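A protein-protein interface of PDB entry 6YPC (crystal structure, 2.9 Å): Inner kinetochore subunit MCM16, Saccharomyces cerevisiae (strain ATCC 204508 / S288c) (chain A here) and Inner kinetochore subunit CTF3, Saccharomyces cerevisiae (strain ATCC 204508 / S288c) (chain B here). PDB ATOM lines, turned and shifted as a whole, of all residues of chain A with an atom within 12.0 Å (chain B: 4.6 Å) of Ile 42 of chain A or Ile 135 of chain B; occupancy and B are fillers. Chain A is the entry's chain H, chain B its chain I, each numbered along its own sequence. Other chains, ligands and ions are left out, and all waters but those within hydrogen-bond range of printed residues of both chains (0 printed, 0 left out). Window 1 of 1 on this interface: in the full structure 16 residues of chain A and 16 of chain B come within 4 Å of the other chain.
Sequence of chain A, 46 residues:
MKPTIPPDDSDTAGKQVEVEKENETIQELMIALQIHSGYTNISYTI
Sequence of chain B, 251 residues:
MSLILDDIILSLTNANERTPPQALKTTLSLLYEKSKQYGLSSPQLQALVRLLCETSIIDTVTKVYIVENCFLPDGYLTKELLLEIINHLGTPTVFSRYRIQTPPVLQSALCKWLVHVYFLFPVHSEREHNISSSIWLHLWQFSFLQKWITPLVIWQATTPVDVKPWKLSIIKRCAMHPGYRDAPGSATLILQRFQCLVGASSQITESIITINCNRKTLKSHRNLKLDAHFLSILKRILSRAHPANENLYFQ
The side-chain carboxylate (OE1) of Glu 28 of chain A sits at hydrogen-bond distance from the side-chain hydroxyl (OG) of Ser 134 of chain B (3.1 Å).
OD1 of Asn 87 of chain B lies close to O of Thr 40 of chain A (3.3 Å).
The side-chain amide oxygen (OD1) of Asn 87 of chain B sits at hydrogen-bond distance from the backbone NH (N) of Asn 41 of chain A, 3.4 Å away.
N of Ile 42 of chain A lies within hydrogen-bond range of OD1 of Asn 87 of chain B, 3.0 Å away.
A ring nitrogen (ND1) of His 36 of chain A sits at hydrogen-bond distance from the backbone carbonyl oxygen (O) of Ala 32 of chain A (3.2 Å).
The backbone NH (N) of Tyr 39 of chain A lies within hydrogen-bond range of the backbone carbonyl oxygen (O) of Gln 34 of chain A (3.0 Å).
The backbone carbonyl oxygen (O) of Leu 83 of chain B sits close to the side-chain amide nitrogen (ND2) of Asn 87 of chain B (3.4 Å).
The backbone carbonyl oxygen (O) of Ile 131 of chain B lies within hydrogen-bond range of the side-chain hydroxyl (OG) of Ser 134 of chain B, 2.8 Å away.
The backbone carbonyl oxygen (O) of Ser 134 of chain B lies within hydrogen-bond range of a ring nitrogen (ND1) of His 138 of chain B (3.2 Å).
Among the printed residues, merely in contact across the chains: Ile 31 of chain A with His 138 of chain B, Ile 31 of chain A with Ser 134 of chain B, Ala 32 of chain A with His 138 of chain B, Tyr 44 of chain A with Ile 131 of chain B, Ser 43 of chain A with Leu 83 of chain B, Ile 35 of chain A with Ile 135 of chain B, Ile 35 of chain A with His 138 of chain B, Gln 27 of chain A with Ile 131 of chain B, His 36 of chain A with His 138 of chain B, Ile 42 of chain A with Leu 83 of chain B, Ile 31 of chain A with Ile 131 of chain B, Tyr 39 of chain A with Asn 87 of chain B and Ile 42 of chain A with Ile 135 of chain B.
Of the printed residues of chain B, Gln 27 of chain A touches Ile 131.
Of the printed residues of chain B, Ile 31 of chain A touches Ile 131 (3.9 Å), Ser 134 (3.5 Å) and His 138 (3.4 Å).
Of the printed residues of chain B, Ile 42 of chain A touches Leu 83 (3.9 Å), Asn 87 (3.0 Å) and Ile 135 (3.996 Å).
Leu 83 of chain B touches just these residues of chain A: Ile 42 (3.9 Å) and Ser 43 (3.6 Å).
No residue of chain A comes within 4 Å of Ile 86 of chain B.
Of chain A, only Gln 27, Ile 31 and Tyr 44 come within 4 Å of Ile 131 of chain B.
No residue of chain A comes within 4 Å of Ser 132 of chain B.
No residue of chain A comes within 4 Å of Ser 133 of chain B.
Ser 134 of chain B touches just these residues of chain A: Glu 28 (3.1 Å) and Ile 31 (3.5 Å).
Of the printed residues of chain A, Ile 135 of chain B touches Ile 35 and Ile 42.
No residue of chain A comes within 4 Å of Trp 136 of chain B.
No residue of chain A comes within 4 Å of Leu 137 of chain B.
His 138 of chain B touches four residues of chain A.
No residue of chain A comes within 4 Å of Leu 139 of chain B.
The nearest printed residue of chain B that does not touch Ile 42 of chain A is Ile 86 of chain B (4.1 Å).
The nearest printed residue of chain A that does not touch Ile 135 of chain B is Ile 31 of chain A (4.2 Å).
Of the 23 printed residues of chain A, 12 touch a printed residue of chain B.
Printed residues of chain A that touch a printed residue of chain B: Gln 27, Glu 28, Ile 31, Ala 32, Ile 35, His 36, Tyr 39, Thr 40, Asn 41, Ile 42, Ser 43 and Tyr 44.
Printed residues of chain B that touch a printed residue of chain A: Leu 83, Asn 87, Ile 131, Ser 134, Ile 135 and His 138.
Among the printed residues, 17 pairs touch across the chains.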
ATOM      1  N   GLU A  24      21.806 -14.115   5.840  1.00  0.00           N
ATOM      2  CA  GLU A  24      20.522 -13.968   6.512  1.00  0.00           C
ATOM      3  C   GLU A  24      20.652 -13.186   7.813  1.00  0.00           C
ATOM      4  O   GLU A  24      19.755 -12.406   8.162  1.00  0.00           O
ATOM      5  CB  GLU A  24      19.875 -15.331   6.773  1.00  0.00           C
ATOM      6  CG  GLU A  24      18.475 -15.213   7.399  1.00  0.00           C
ATOM      7  CD  GLU A  24      17.560 -14.195   6.659  1.00  0.00           C
ATOM      8  OE1 GLU A  24      17.607 -14.108   5.395  1.00  0.00           O
ATOM      9  OE2 GLU A  24      16.790 -13.475   7.349  1.00  0.00           O
ATOM     10  N   THR A  25      21.745 -13.361   8.553  1.00  0.00           N
ATOM     11  CA  THR A  25      21.760 -12.668   9.831  1.00  0.00           C
ATOM     12  C   THR A  25      22.045 -11.176   9.665  1.00  0.00           C
ATOM     13  O   THR A  25      21.376 -10.358  10.304  1.00  0.00           O
ATOM     14  CB  THR A  25      22.746 -13.328  10.788  1.00  0.00           C
ATOM     15  OG1 THR A  25      24.077 -13.002  10.391  1.00  0.00           O
ATOM     16  CG2 THR A  25      22.572 -14.824  10.769  1.00  0.00           C
ATOM     17  N   ILE A  26      23.005 -10.789   8.813  1.00  0.00           N
ATOM     18  CA  ILE A  26      23.227  -9.362   8.553  1.00  0.00           C
ATOM     19  C   ILE A  26      21.914  -8.680   8.201  1.00  0.00           C
ATOM     20  O   ILE A  26      21.583  -7.610   8.727  1.00  0.00           O
ATOM     21  CB  ILE A  26      24.251  -9.150   7.428  1.00  0.00           C
ATOM     22  CG1 ILE A  26      25.605  -9.781   7.777  1.00  0.00           C
ATOM     23  CG2 ILE A  26      24.376  -7.651   7.138  1.00  0.00           C
ATOM     24  CD1 ILE A  26      26.674  -9.633   6.648  1.00  0.00           C
ATOM     25  N   GLN A  27      21.148  -9.289   7.296  1.00  0.00           N
ATOM     26  CA  GLN A  27      19.852  -8.733   6.936  1.00  0.00           C
ATOM     27  C   GLN A  27      18.988  -8.542   8.176  1.00  0.00           C
ATOM     28  O   GLN A  27      18.558  -7.426   8.489  1.00  0.00           O
ATOM     29  CB  GLN A  27      19.149  -9.631   5.913  1.00  0.00           C
ATOM     30  CG  GLN A  27      17.909  -8.993   5.278  1.00  0.00           C
ATOM     31  CD  GLN A  27      17.332  -9.796   4.105  1.00  0.00           C
ATOM     32  OE1 GLN A  27      17.845  -9.740   2.980  1.00  0.00           O
ATOM     33  NE2 GLN A  27      16.253 -10.538   4.366  1.00  0.00           N
ATOM     34  N   GLU A  28      18.746  -9.618   8.918  1.00  0.00           N
ATOM     35  CA  GLU A  28      17.885  -9.476  10.081  1.00  0.00           C
ATOM     36  C   GLU A  28      18.497  -8.579  11.144  1.00  0.00           C
ATOM     37  O   GLU A  28      17.753  -7.977  11.923  1.00  0.00           O
ATOM     38  CB  GLU A  28      17.561 -10.850  10.653  1.00  0.00           C
ATOM     39  CG  GLU A  28      16.538 -11.628   9.810  1.00  0.00           C
ATOM     40  CD  GLU A  28      15.232 -10.858   9.606  1.00  0.00           C
ATOM     41  OE1 GLU A  28      14.614 -10.975   8.506  1.00  0.00           O
ATOM     42  OE2 GLU A  28      14.841 -10.120  10.547  1.00  0.00           O
ATOM     43  N   LEU A  29      19.826  -8.457  11.175  1.00  0.00           N
ATOM     44  CA  LEU A  29      20.478  -7.583  12.145  1.00  0.00           C
ATOM     45  C   LEU A  29      20.210  -6.121  11.821  1.00  0.00           C
ATOM     46  O   LEU A  29      19.864  -5.329  12.710  1.00  0.00           O
ATOM     47  CB  LEU A  29      21.983  -7.862  12.180  1.00  0.00           C
ATOM     48  CG  LEU A  29      22.892  -7.058  13.117  1.00  0.00           C
ATOM     49  CD1 LEU A  29      22.580  -7.317  14.591  1.00  0.00           C
ATOM     50  CD2 LEU A  29      24.335  -7.422  12.852  1.00  0.00           C
ATOM     51  N   MET A  30      20.336  -5.746  10.543  1.00  0.00           N
ATOM     52  CA  MET A  30      20.147  -4.347  10.183  1.00  0.00           C
ATOM     53  C   MET A  30      18.723  -3.896  10.486  1.00  0.00           C
ATOM     54  O   MET A  30      18.516  -2.897  11.185  1.00  0.00           O
ATOM     55  CB  MET A  30      20.516  -4.121   8.718  1.00  0.00           C
ATOM     56  CG  MET A  30      21.966  -4.475   8.410  1.00  0.00           C
ATOM     57  SD  MET A  30      22.690  -3.524   7.046  1.00  0.00           S
ATOM     58  CE  MET A  30      22.505  -1.841   7.633  1.00  0.00           C
ATOM     59  N   ILE A  31      17.731  -4.632  10.003  1.00  0.00           N
ATOM     60  CA  ILE A  31      16.338  -4.334  10.325  1.00  0.00           C
ATOM     61  C   ILE A  31      16.189  -3.992  11.807  1.00  0.00           C
ATOM     62  O   ILE A  31      15.465  -3.062  12.186  1.00  0.00           O
ATOM     63  CB  ILE A  31      15.435  -5.525   9.952  1.00  0.00           C
ATOM     64  CG1 ILE A  31      15.161  -5.535   8.453  1.00  0.00           C
ATOM     65  CG2 ILE A  31      14.150  -5.540  10.795  1.00  0.00           C
ATOM     66  CD1 ILE A  31      14.803  -6.899   7.939  1.00  0.00           C
ATOM     67  N   ALA A  32      16.875  -4.722  12.669  1.00  0.00           N
ATOM     68  CA  ALA A  32      16.596  -4.460  14.060  1.00  0.00           C
ATOM     69  C   ALA A  32      17.349  -3.232  14.534  1.00  0.00           C
ATOM     70  O   ALA A  32      16.810  -2.453  15.329  1.00  0.00           O
ATOM     71  CB  ALA A  32      16.926  -5.686  14.903  1.00  0.00           C
ATOM     72  N   LEU A  33      18.585  -3.040  14.063  1.00  0.00           N
ATOM     73  CA  LEU A  33      19.296  -1.797  14.350  1.00  0.00           C
ATOM     74  C   LEU A  33      18.501  -0.594  13.841  1.00  0.00           C
ATOM     75  O   LEU A  33      18.233   0.363  14.580  1.00  0.00           O
ATOM     76  CB  LEU A  33      20.677  -1.829  13.703  1.00  0.00           C
ATOM     77  CG  LEU A  33      21.673  -2.917  14.144  1.00  0.00           C
ATOM     78  CD1 LEU A  33      22.926  -2.968  13.265  1.00  0.00           C
ATOM     79  CD2 LEU A  33      22.072  -2.753  15.603  1.00  0.00           C
ATOM     80  N   GLN A  34      18.080  -0.645  12.580  1.00  0.00           N
ATOM     81  CA  GLN A  34      17.385   0.492  12.001  1.00  0.00           C
ATOM     82  C   GLN A  34      16.132   0.841  12.791  1.00  0.00           C
ATOM     83  O   GLN A  34      15.904   2.006  13.135  1.00  0.00           O
ATOM     84  CB  GLN A  34      17.060   0.193  10.548  1.00  0.00           C
ATOM     85  CG  GLN A  34      18.314   0.086   9.738  1.00  0.00           C
ATOM     86  CD  GLN A  34      18.046  -0.077   8.261  1.00  0.00           C
ATOM     87  OE1 GLN A  34      16.890  -0.182   7.829  1.00  0.00           O
ATOM     88  NE2 GLN A  34      19.117  -0.122   7.468  1.00  0.00           N
ATOM     89  N   ILE A  35      15.309  -0.152  13.094  1.00  0.00           N
ATOM     90  CA  ILE A  35      14.040   0.135  13.747  1.00  0.00           C
ATOM     91  C   ILE A  35      14.269   0.729  15.123  1.00  0.00           C
ATOM     92  O   ILE A  35      13.636   1.720  15.507  1.00  0.00           O
ATOM     93  CB  ILE A  35      13.196  -1.136  13.846  1.00  0.00           C
ATOM     94  CG1 ILE A  35      12.741  -1.533  12.454  1.00  0.00           C
ATOM     95  CG2 ILE A  35      12.054  -0.922  14.864  1.00  0.00           C
ATOM     96  CD1 ILE A  35      11.564  -2.435  12.479  1.00  0.00           C
ATOM     97  N   HIS A  36      15.154   0.130  15.887  1.00  0.00           N
ATOM     98  CA  HIS A  36      15.263   0.497  17.280  1.00  0.00           C
ATOM     99  C   HIS A  36      16.285   1.581  17.509  1.00  0.00           C
ATOM    100  O   HIS A  36      16.575   1.901  18.667  1.00  0.00           O
ATOM    101  CB  HIS A  36      15.607  -0.726  18.110  1.00  0.00           C
ATOM    102  CG  HIS A  36      14.491  -1.713  18.189  1.00  0.00           C
ATOM    103  ND1 HIS A  36      14.402  -2.804  17.352  1.00  0.00           N
ATOM    104  CD2 HIS A  36      13.402  -1.763  18.996  1.00  0.00           C
ATOM    105  CE1 HIS A  36      13.313  -3.494  17.652  1.00  0.00           C
ATOM    106  NE2 HIS A  36      12.693  -2.889  18.650  1.00  0.00           N
ATOM    107  N   SER A  37      16.866   2.127  16.448  1.00  0.00           N
ATOM    108  CA  SER A  37      17.668   3.335  16.562  1.00  0.00           C
ATOM    109  C   SER A  37      16.975   4.512  15.891  1.00  0.00           C
ATOM    110  O   SER A  37      17.622   5.520  15.583  1.00  0.00           O
ATOM    111  CB  SER A  37      19.067   3.123  15.982  1.00  0.00           C
ATOM    112  OG  SER A  37      19.032   2.784  14.602  1.00  0.00           O
ATOM    113  N   GLY A  38      15.667   4.389  15.653  1.00  0.00           N
ATOM    114  CA  GLY A  38      14.901   5.460  15.060  1.00  0.00           C
ATOM    115  C   GLY A  38      15.331   5.873  13.671  1.00  0.00           C
ATOM    116  O   GLY A  38      15.023   6.996  13.258  1.00  0.00           O
ATOM    117  N   TYR A  39      16.050   5.011  12.939  1.00  0.00           N
ATOM    118  CA  TYR A  39      16.413   5.318  11.559  1.00  0.00           C
ATOM    119  C   TYR A  39      15.151   5.572  10.762  1.00  0.00           C
ATOM    120  O   TYR A  39      14.120   4.947  11.006  1.00  0.00           O
ATOM    121  CB  TYR A  39      17.179   4.164  10.937  1.00  0.00           C
ATOM    122  CG  TYR A  39      17.947   4.450   9.666  1.00  0.00           C
ATOM    123  CD1 TYR A  39      19.014   5.341   9.648  1.00  0.00           C
ATOM    124  CD2 TYR A  39      17.656   3.762   8.502  1.00  0.00           C
ATOM    125  CE1 TYR A  39      19.749   5.565   8.475  1.00  0.00           C
ATOM    126  CE2 TYR A  39      18.370   3.970   7.339  1.00  0.00           C
ATOM    127  CZ  TYR A  39      19.414   4.870   7.323  1.00  0.00           C
ATOM    128  OH  TYR A  39      20.111   5.078   6.144  1.00  0.00           O
ATOM    129  N   THR A  40      15.223   6.513   9.822  1.00  0.00           N
ATOM    130  CA  THR A  40      14.041   6.939   9.079  1.00  0.00           C
ATOM    131  C   THR A  40      14.216   6.764   7.580  1.00  0.00           C
ATOM    132  O   THR A  40      13.493   7.395   6.802  1.00  0.00           O
ATOM    133  CB  THR A  40      13.723   8.392   9.378  1.00  0.00           C
ATOM    134  OG1 THR A  40      14.861   9.184   9.037  1.00  0.00           O
ATOM    135  CG2 THR A  40      13.447   8.566  10.845  1.00  0.00           C
ATOM    136  N   ASN A  41      15.182   5.938   7.159  1.00  0.00           N
ATOM    137  CA  ASN A  41      15.390   5.625   5.752  1.00  0.00           C
ATOM    138  C   ASN A  41      15.361   4.110   5.527  1.00  0.00           C
ATOM    139  O   ASN A  41      15.943   3.593   4.560  1.00  0.00           O
ATOM    140  CB  ASN A  41      16.680   6.267   5.241  1.00  0.00           C
ATOM    141  CG  ASN A  41      16.864   6.084   3.750  1.00  0.00           C
ATOM    142  OD1 ASN A  41      15.902   6.150   2.977  1.00  0.00           O
ATOM    143  ND2 ASN A  41      18.106   5.845   3.334  1.00  0.00           N
ATOM    144  N   ILE A  42      14.652   3.399   6.411  1.00  0.00           N
ATOM    145  CA  ILE A  42      14.346   1.980   6.234  1.00  0.00           C
ATOM    146  C   ILE A  42      13.764   1.715   4.863  1.00  0.00           C
ATOM    147  O   ILE A  42      12.702   2.249   4.532  1.00  0.00           O
ATOM    148  CB  ILE A  42      13.329   1.531   7.288  1.00  0.00           C
ATOM    149  CG1 ILE A  42      13.873   1.679   8.691  1.00  0.00           C
ATOM    150  CG2 ILE A  42      12.863   0.140   6.989  1.00  0.00           C
ATOM    151  CD1 ILE A  42      12.868   1.258   9.710  1.00  0.00           C
ATOM    152  N   SER A  43      14.410   0.839   4.083  1.00  0.00           N
ATOM    153  CA  SER A  43      13.934   0.502   2.737  1.00  0.00           C
ATOM    154  C   SER A  43      13.976  -0.994   2.461  1.00  0.00           C
ATOM    155  O   SER A  43      13.687  -1.805   3.339  1.00  0.00           O
ATOM    156  CB  SER A  43      14.774   1.213   1.675  1.00  0.00           C
ATOM    157  OG  SER A  43      16.091   0.689   1.654  1.00  0.00           O
ATOM    158  N   TYR A  44      14.321  -1.367   1.234  1.00  0.00           N
ATOM    159  CA  TYR A  44      14.695  -2.736   0.900  1.00  0.00           C
ATOM    160  C   TYR A  44      16.022  -2.666   0.142  1.00  0.00           C
ATOM    161  O   TYR A  44      16.069  -2.212  -1.008  1.00  0.00           O
ATOM    162  CB  TYR A  44      13.612  -3.428   0.080  1.00  0.00           C
ATOM    163  CG  TYR A  44      12.169  -3.451   0.628  1.00  0.00           C
ATOM    164  CD1 TYR A  44      11.878  -3.926   1.886  1.00  0.00           C
ATOM    165  CD2 TYR A  44      11.088  -3.086  -0.175  1.00  0.00           C
ATOM    166  CE1 TYR A  44      10.540  -3.988   2.356  1.00  0.00           C
ATOM    167  CE2 TYR A  44       9.760  -3.147   0.282  1.00  0.00           C
ATOM    168  CZ  TYR A  44       9.489  -3.593   1.545  1.00  0.00           C
ATOM    169  OH  TYR A  44       8.176  -3.647   2.004  1.00  0.00           O
ATOM    170  N   THR A  45      17.108  -3.052   0.809  1.00  0.00           N
ATOM    171  CA  THR A  45      18.444  -3.083   0.220  1.00  0.00           C
ATOM    172  C   THR A  45      18.746  -4.473  -0.346  1.00  0.00           C
ATOM    173  O   THR A  45      18.325  -5.491   0.221  1.00  0.00           O
ATOM    174  CB  THR A  45      19.510  -2.702   1.257  1.00  0.00           C
ATOM    175  OG1 THR A  45      20.818  -2.897   0.699  1.00  0.00           O
ATOM    176  CG2 THR A  45      19.374  -3.555   2.535  1.00  0.00           C
ATOM    177  N   ILE A  46      19.471  -4.512  -1.475  1.00  0.00           N
ATOM    178  CA  ILE A  46      19.873  -5.780  -2.114  1.00  0.00           C
ATOM    179  C   ILE A  46      21.196  -6.283  -1.507  1.00  0.00           C
ATOM    180  O   ILE A  46      21.205  -6.977  -0.479  1.00  0.00           O
ATOM    181  CB  ILE A  46      19.981  -5.638  -3.673  1.00  0.00           C
ATOM    182  CG1 ILE A  46      20.015  -7.016  -4.351  1.00  0.00           C
ATOM    183  CG2 ILE A  46      21.200  -4.803  -4.074  1.00  0.00           C
ATOM    184  CD1 ILE A  46      20.404  -6.972  -5.818  1.00  0.00           C
ATOM    185  N   LEU B  83       6.732   2.142   3.077  1.00  0.00           N
ATOM    186  CA  LEU B  83       7.981   2.607   3.666  1.00  0.00           C
ATOM    187  C   LEU B  83       7.788   3.959   4.329  1.00  0.00           C
ATOM    188  O   LEU B  83       8.252   4.171   5.458  1.00  0.00           O
ATOM    189  CB  LEU B  83       9.077   2.653   2.617  1.00  0.00           C
ATOM    190  CG  LEU B  83       9.347   1.245   2.111  1.00  0.00           C
ATOM    191  CD1 LEU B  83      10.654   1.212   1.381  1.00  0.00           C
ATOM    192  CD2 LEU B  83       9.366   0.278   3.270  1.00  0.00           C
ATOM    193  N   ILE B  86       6.082   3.297   7.512  1.00  0.00           N
ATOM    194  CA  ILE B  86       6.979   2.610   8.443  1.00  0.00           C
ATOM    195  C   ILE B  86       7.983   3.592   9.026  1.00  0.00           C
ATOM    196  O   ILE B  86       8.228   3.619  10.238  1.00  0.00           O
ATOM    197  CB  ILE B  86       7.714   1.448   7.750  1.00  0.00           C
ATOM    198  CG1 ILE B  86       6.785   0.269   7.481  1.00  0.00           C
ATOM    199  CG2 ILE B  86       8.919   1.007   8.585  1.00  0.00           C
ATOM    200  CD1 ILE B  86       7.150  -0.454   6.174  1.00  0.00           C
ATOM    201  N   ASN B  87       8.577   4.411   8.166  1.00  0.00           N
ATOM    202  CA  ASN B  87       9.619   5.298   8.624  1.00  0.00           C
ATOM    203  C   ASN B  87       9.087   6.322   9.622  1.00  0.00           C
ATOM    204  O   ASN B  87       9.866   7.073  10.208  1.00  0.00           O
ATOM    205  CB  ASN B  87      10.270   5.958   7.425  1.00  0.00           C
ATOM    206  CG  ASN B  87      11.363   5.109   6.851  1.00  0.00           C
ATOM    207  OD1 ASN B  87      12.104   4.500   7.594  1.00  0.00           O
ATOM    208  ND2 ASN B  87      11.482   5.071   5.535  1.00  0.00           N
ATOM    209  N   ILE B 131      11.702  -9.424   4.519  1.00  0.00           N
ATOM    210  CA  ILE B 131      11.990  -8.181   5.221  1.00  0.00           C
ATOM    211  C   ILE B 131      10.723  -7.662   5.871  1.00  0.00           C
ATOM    212  O   ILE B 131      10.618  -7.577   7.103  1.00  0.00           O
ATOM    213  CB  ILE B 131      12.593  -7.143   4.259  1.00  0.00           C
ATOM    214  CG1 ILE B 131      14.009  -7.548   3.860  1.00  0.00           C
ATOM    215  CG2 ILE B 131      12.622  -5.769   4.897  1.00  0.00           C
ATOM    216  CD1 ILE B 131      14.616  -6.629   2.809  1.00  0.00           C
ATOM    217  N   SER B 132       9.724  -7.356   5.044  1.00  0.00           N
ATOM    218  CA  SER B 132       8.466  -6.867   5.574  1.00  0.00           C
ATOM    219  C   SER B 132       7.948  -7.735   6.712  1.00  0.00           C
ATOM    220  O   SER B 132       7.326  -7.224   7.643  1.00  0.00           O
ATOM    221  CB  SER B 132       7.419  -6.814   4.490  1.00  0.00           C
ATOM    222  OG  SER B 132       6.142  -6.909   5.085  1.00  0.00           O
ATOM    223  N   SER B 133       8.202  -9.042   6.686  1.00  0.00           N
ATOM    224  CA  SER B 133       7.625  -9.869   7.735  1.00  0.00           C
ATOM    225  C   SER B 133       8.311  -9.612   9.055  1.00  0.00           C
ATOM    226  O   SER B 133       7.669  -9.684  10.109  1.00  0.00           O
ATOM    227  CB  SER B 133       7.719 -11.340   7.361  1.00  0.00           C
ATOM    228  OG  SER B 133       8.975 -11.591   6.760  1.00  0.00           O
ATOM    229  N   SER B 134       9.595  -9.286   9.020  1.00  0.00           N
ATOM    230  CA  SER B 134      10.302  -9.087  10.278  1.00  0.00           C
ATOM    231  C   SER B 134      10.125  -7.671  10.818  1.00  0.00           C
ATOM    232  O   SER B 134      10.084  -7.468  12.033  1.00  0.00           O
ATOM    233  CB  SER B 134      11.778  -9.415  10.103  1.00  0.00           C
ATOM    234  OG  SER B 134      12.221  -9.073   8.816  1.00  0.00           O
ATOM    235  N   ILE B 135      10.005  -6.673   9.938  1.00  0.00           N
ATOM    236  CA  ILE B 135       9.719  -5.310  10.393  1.00  0.00           C
ATOM    237  C   ILE B 135       8.470  -5.302  11.256  1.00  0.00           C
ATOM    238  O   ILE B 135       8.493  -4.865  12.409  1.00  0.00           O
ATOM    239  CB  ILE B 135       9.559  -4.352   9.205  1.00  0.00           C
ATOM    240  CG1 ILE B 135      10.872  -4.212   8.443  1.00  0.00           C
ATOM    241  CG2 ILE B 135       9.133  -3.036   9.753  1.00  0.00           C
ATOM    242  CD1 ILE B 135      10.777  -3.259   7.242  1.00  0.00           C
ATOM    243  N   TRP B 136       7.364  -5.810  10.717  1.00  0.00           N
ATOM    244  CA  TRP B 136       6.116  -5.770  11.467  1.00  0.00           C
ATOM    245  C   TRP B 136       6.199  -6.568  12.755  1.00  0.00           C
ATOM    246  O   TRP B 136       5.558  -6.221  13.756  1.00  0.00           O
ATOM    247  CB  TRP B 136       4.986  -6.277  10.601  1.00  0.00           C
ATOM    248  CG  TRP B 136       4.772  -5.389   9.443  1.00  0.00           C
ATOM    249  CD1 TRP B 136       5.040  -5.661   8.138  1.00  0.00           C
ATOM    250  CD2 TRP B 136       4.271  -4.061   9.481  1.00  0.00           C
ATOM    251  NE1 TRP B 136       4.731  -4.579   7.349  1.00  0.00           N
ATOM    252  CE2 TRP B 136       4.250  -3.582   8.154  1.00  0.00           C
ATOM    253  CE3 TRP B 136       3.830  -3.229  10.504  1.00  0.00           C
ATOM    254  CZ2 TRP B 136       3.796  -2.315   7.828  1.00  0.00           C
ATOM    255  CZ3 TRP B 136       3.367  -1.972  10.178  1.00  0.00           C
ATOM    256  CH2 TRP B 136       3.355  -1.525   8.852  1.00  0.00           C
ATOM    257  N   LEU B 137       6.989  -7.629  12.769  1.00  0.00           N
ATOM    258  CA  LEU B 137       7.118  -8.345  14.021  1.00  0.00           C
ATOM    259  C   LEU B 137       7.860  -7.496  15.041  1.00  0.00           C
ATOM    260  O   LEU B 137       7.465  -7.434  16.215  1.00  0.00           O
ATOM    261  CB  LEU B 137       7.827  -9.672  13.805  1.00  0.00           C
ATOM    262  CG  LEU B 137       7.836 -10.403  15.137  1.00  0.00           C
ATOM    263  CD1 LEU B 137       6.406 -10.766  15.550  1.00  0.00           C
ATOM    264  CD2 LEU B 137       8.743 -11.603  15.054  1.00  0.00           C
ATOM    265  N   HIS B 138       8.939  -6.840  14.602  1.00  0.00           N
ATOM    266  CA  HIS B 138       9.667  -5.921  15.467  1.00  0.00           C
ATOM    267  C   HIS B 138       8.759  -4.793  15.940  1.00  0.00           C
ATOM    268  O   HIS B 138       8.660  -4.525  17.143  1.00  0.00           O
ATOM    269  CB  HIS B 138      10.866  -5.362  14.719  1.00  0.00           C
ATOM    270  CG  HIS B 138      12.076  -6.243  14.764  1.00  0.00           C
ATOM    271  ND1 HIS B 138      12.731  -6.665  13.626  1.00  0.00           N
ATOM    272  CD2 HIS B 138      12.778  -6.748  15.807  1.00  0.00           C
ATOM    273  CE1 HIS B 138      13.781  -7.395  13.962  1.00  0.00           C
ATOM    274  NE2 HIS B 138      13.831  -7.462  15.281  1.00  0.00           N
ATOM    275  N   LEU B 139       8.057  -4.148  14.998  1.00  0.00           N
ATOM    276  CA  LEU B 139       7.104  -3.087  15.328  1.00  0.00           C
ATOM    277  C   LEU B 139       6.008  -3.578  16.253  1.00  0.00           C
ATOM    278  O   LEU B 139       5.539  -2.838  17.125  1.00  0.00           O
ATOM    279  CB  LEU B 139       6.471  -2.540  14.059  1.00  0.00           C
ATOM    280  CG  LEU B 139       7.377  -1.610  13.274  1.00  0.00           C
ATOM    281  CD1 LEU B 139       6.580  -0.904  12.198  1.00  0.00           C
ATOM    282  CD2 LEU B 139       8.012  -0.622  14.232  1.00  0.00           C
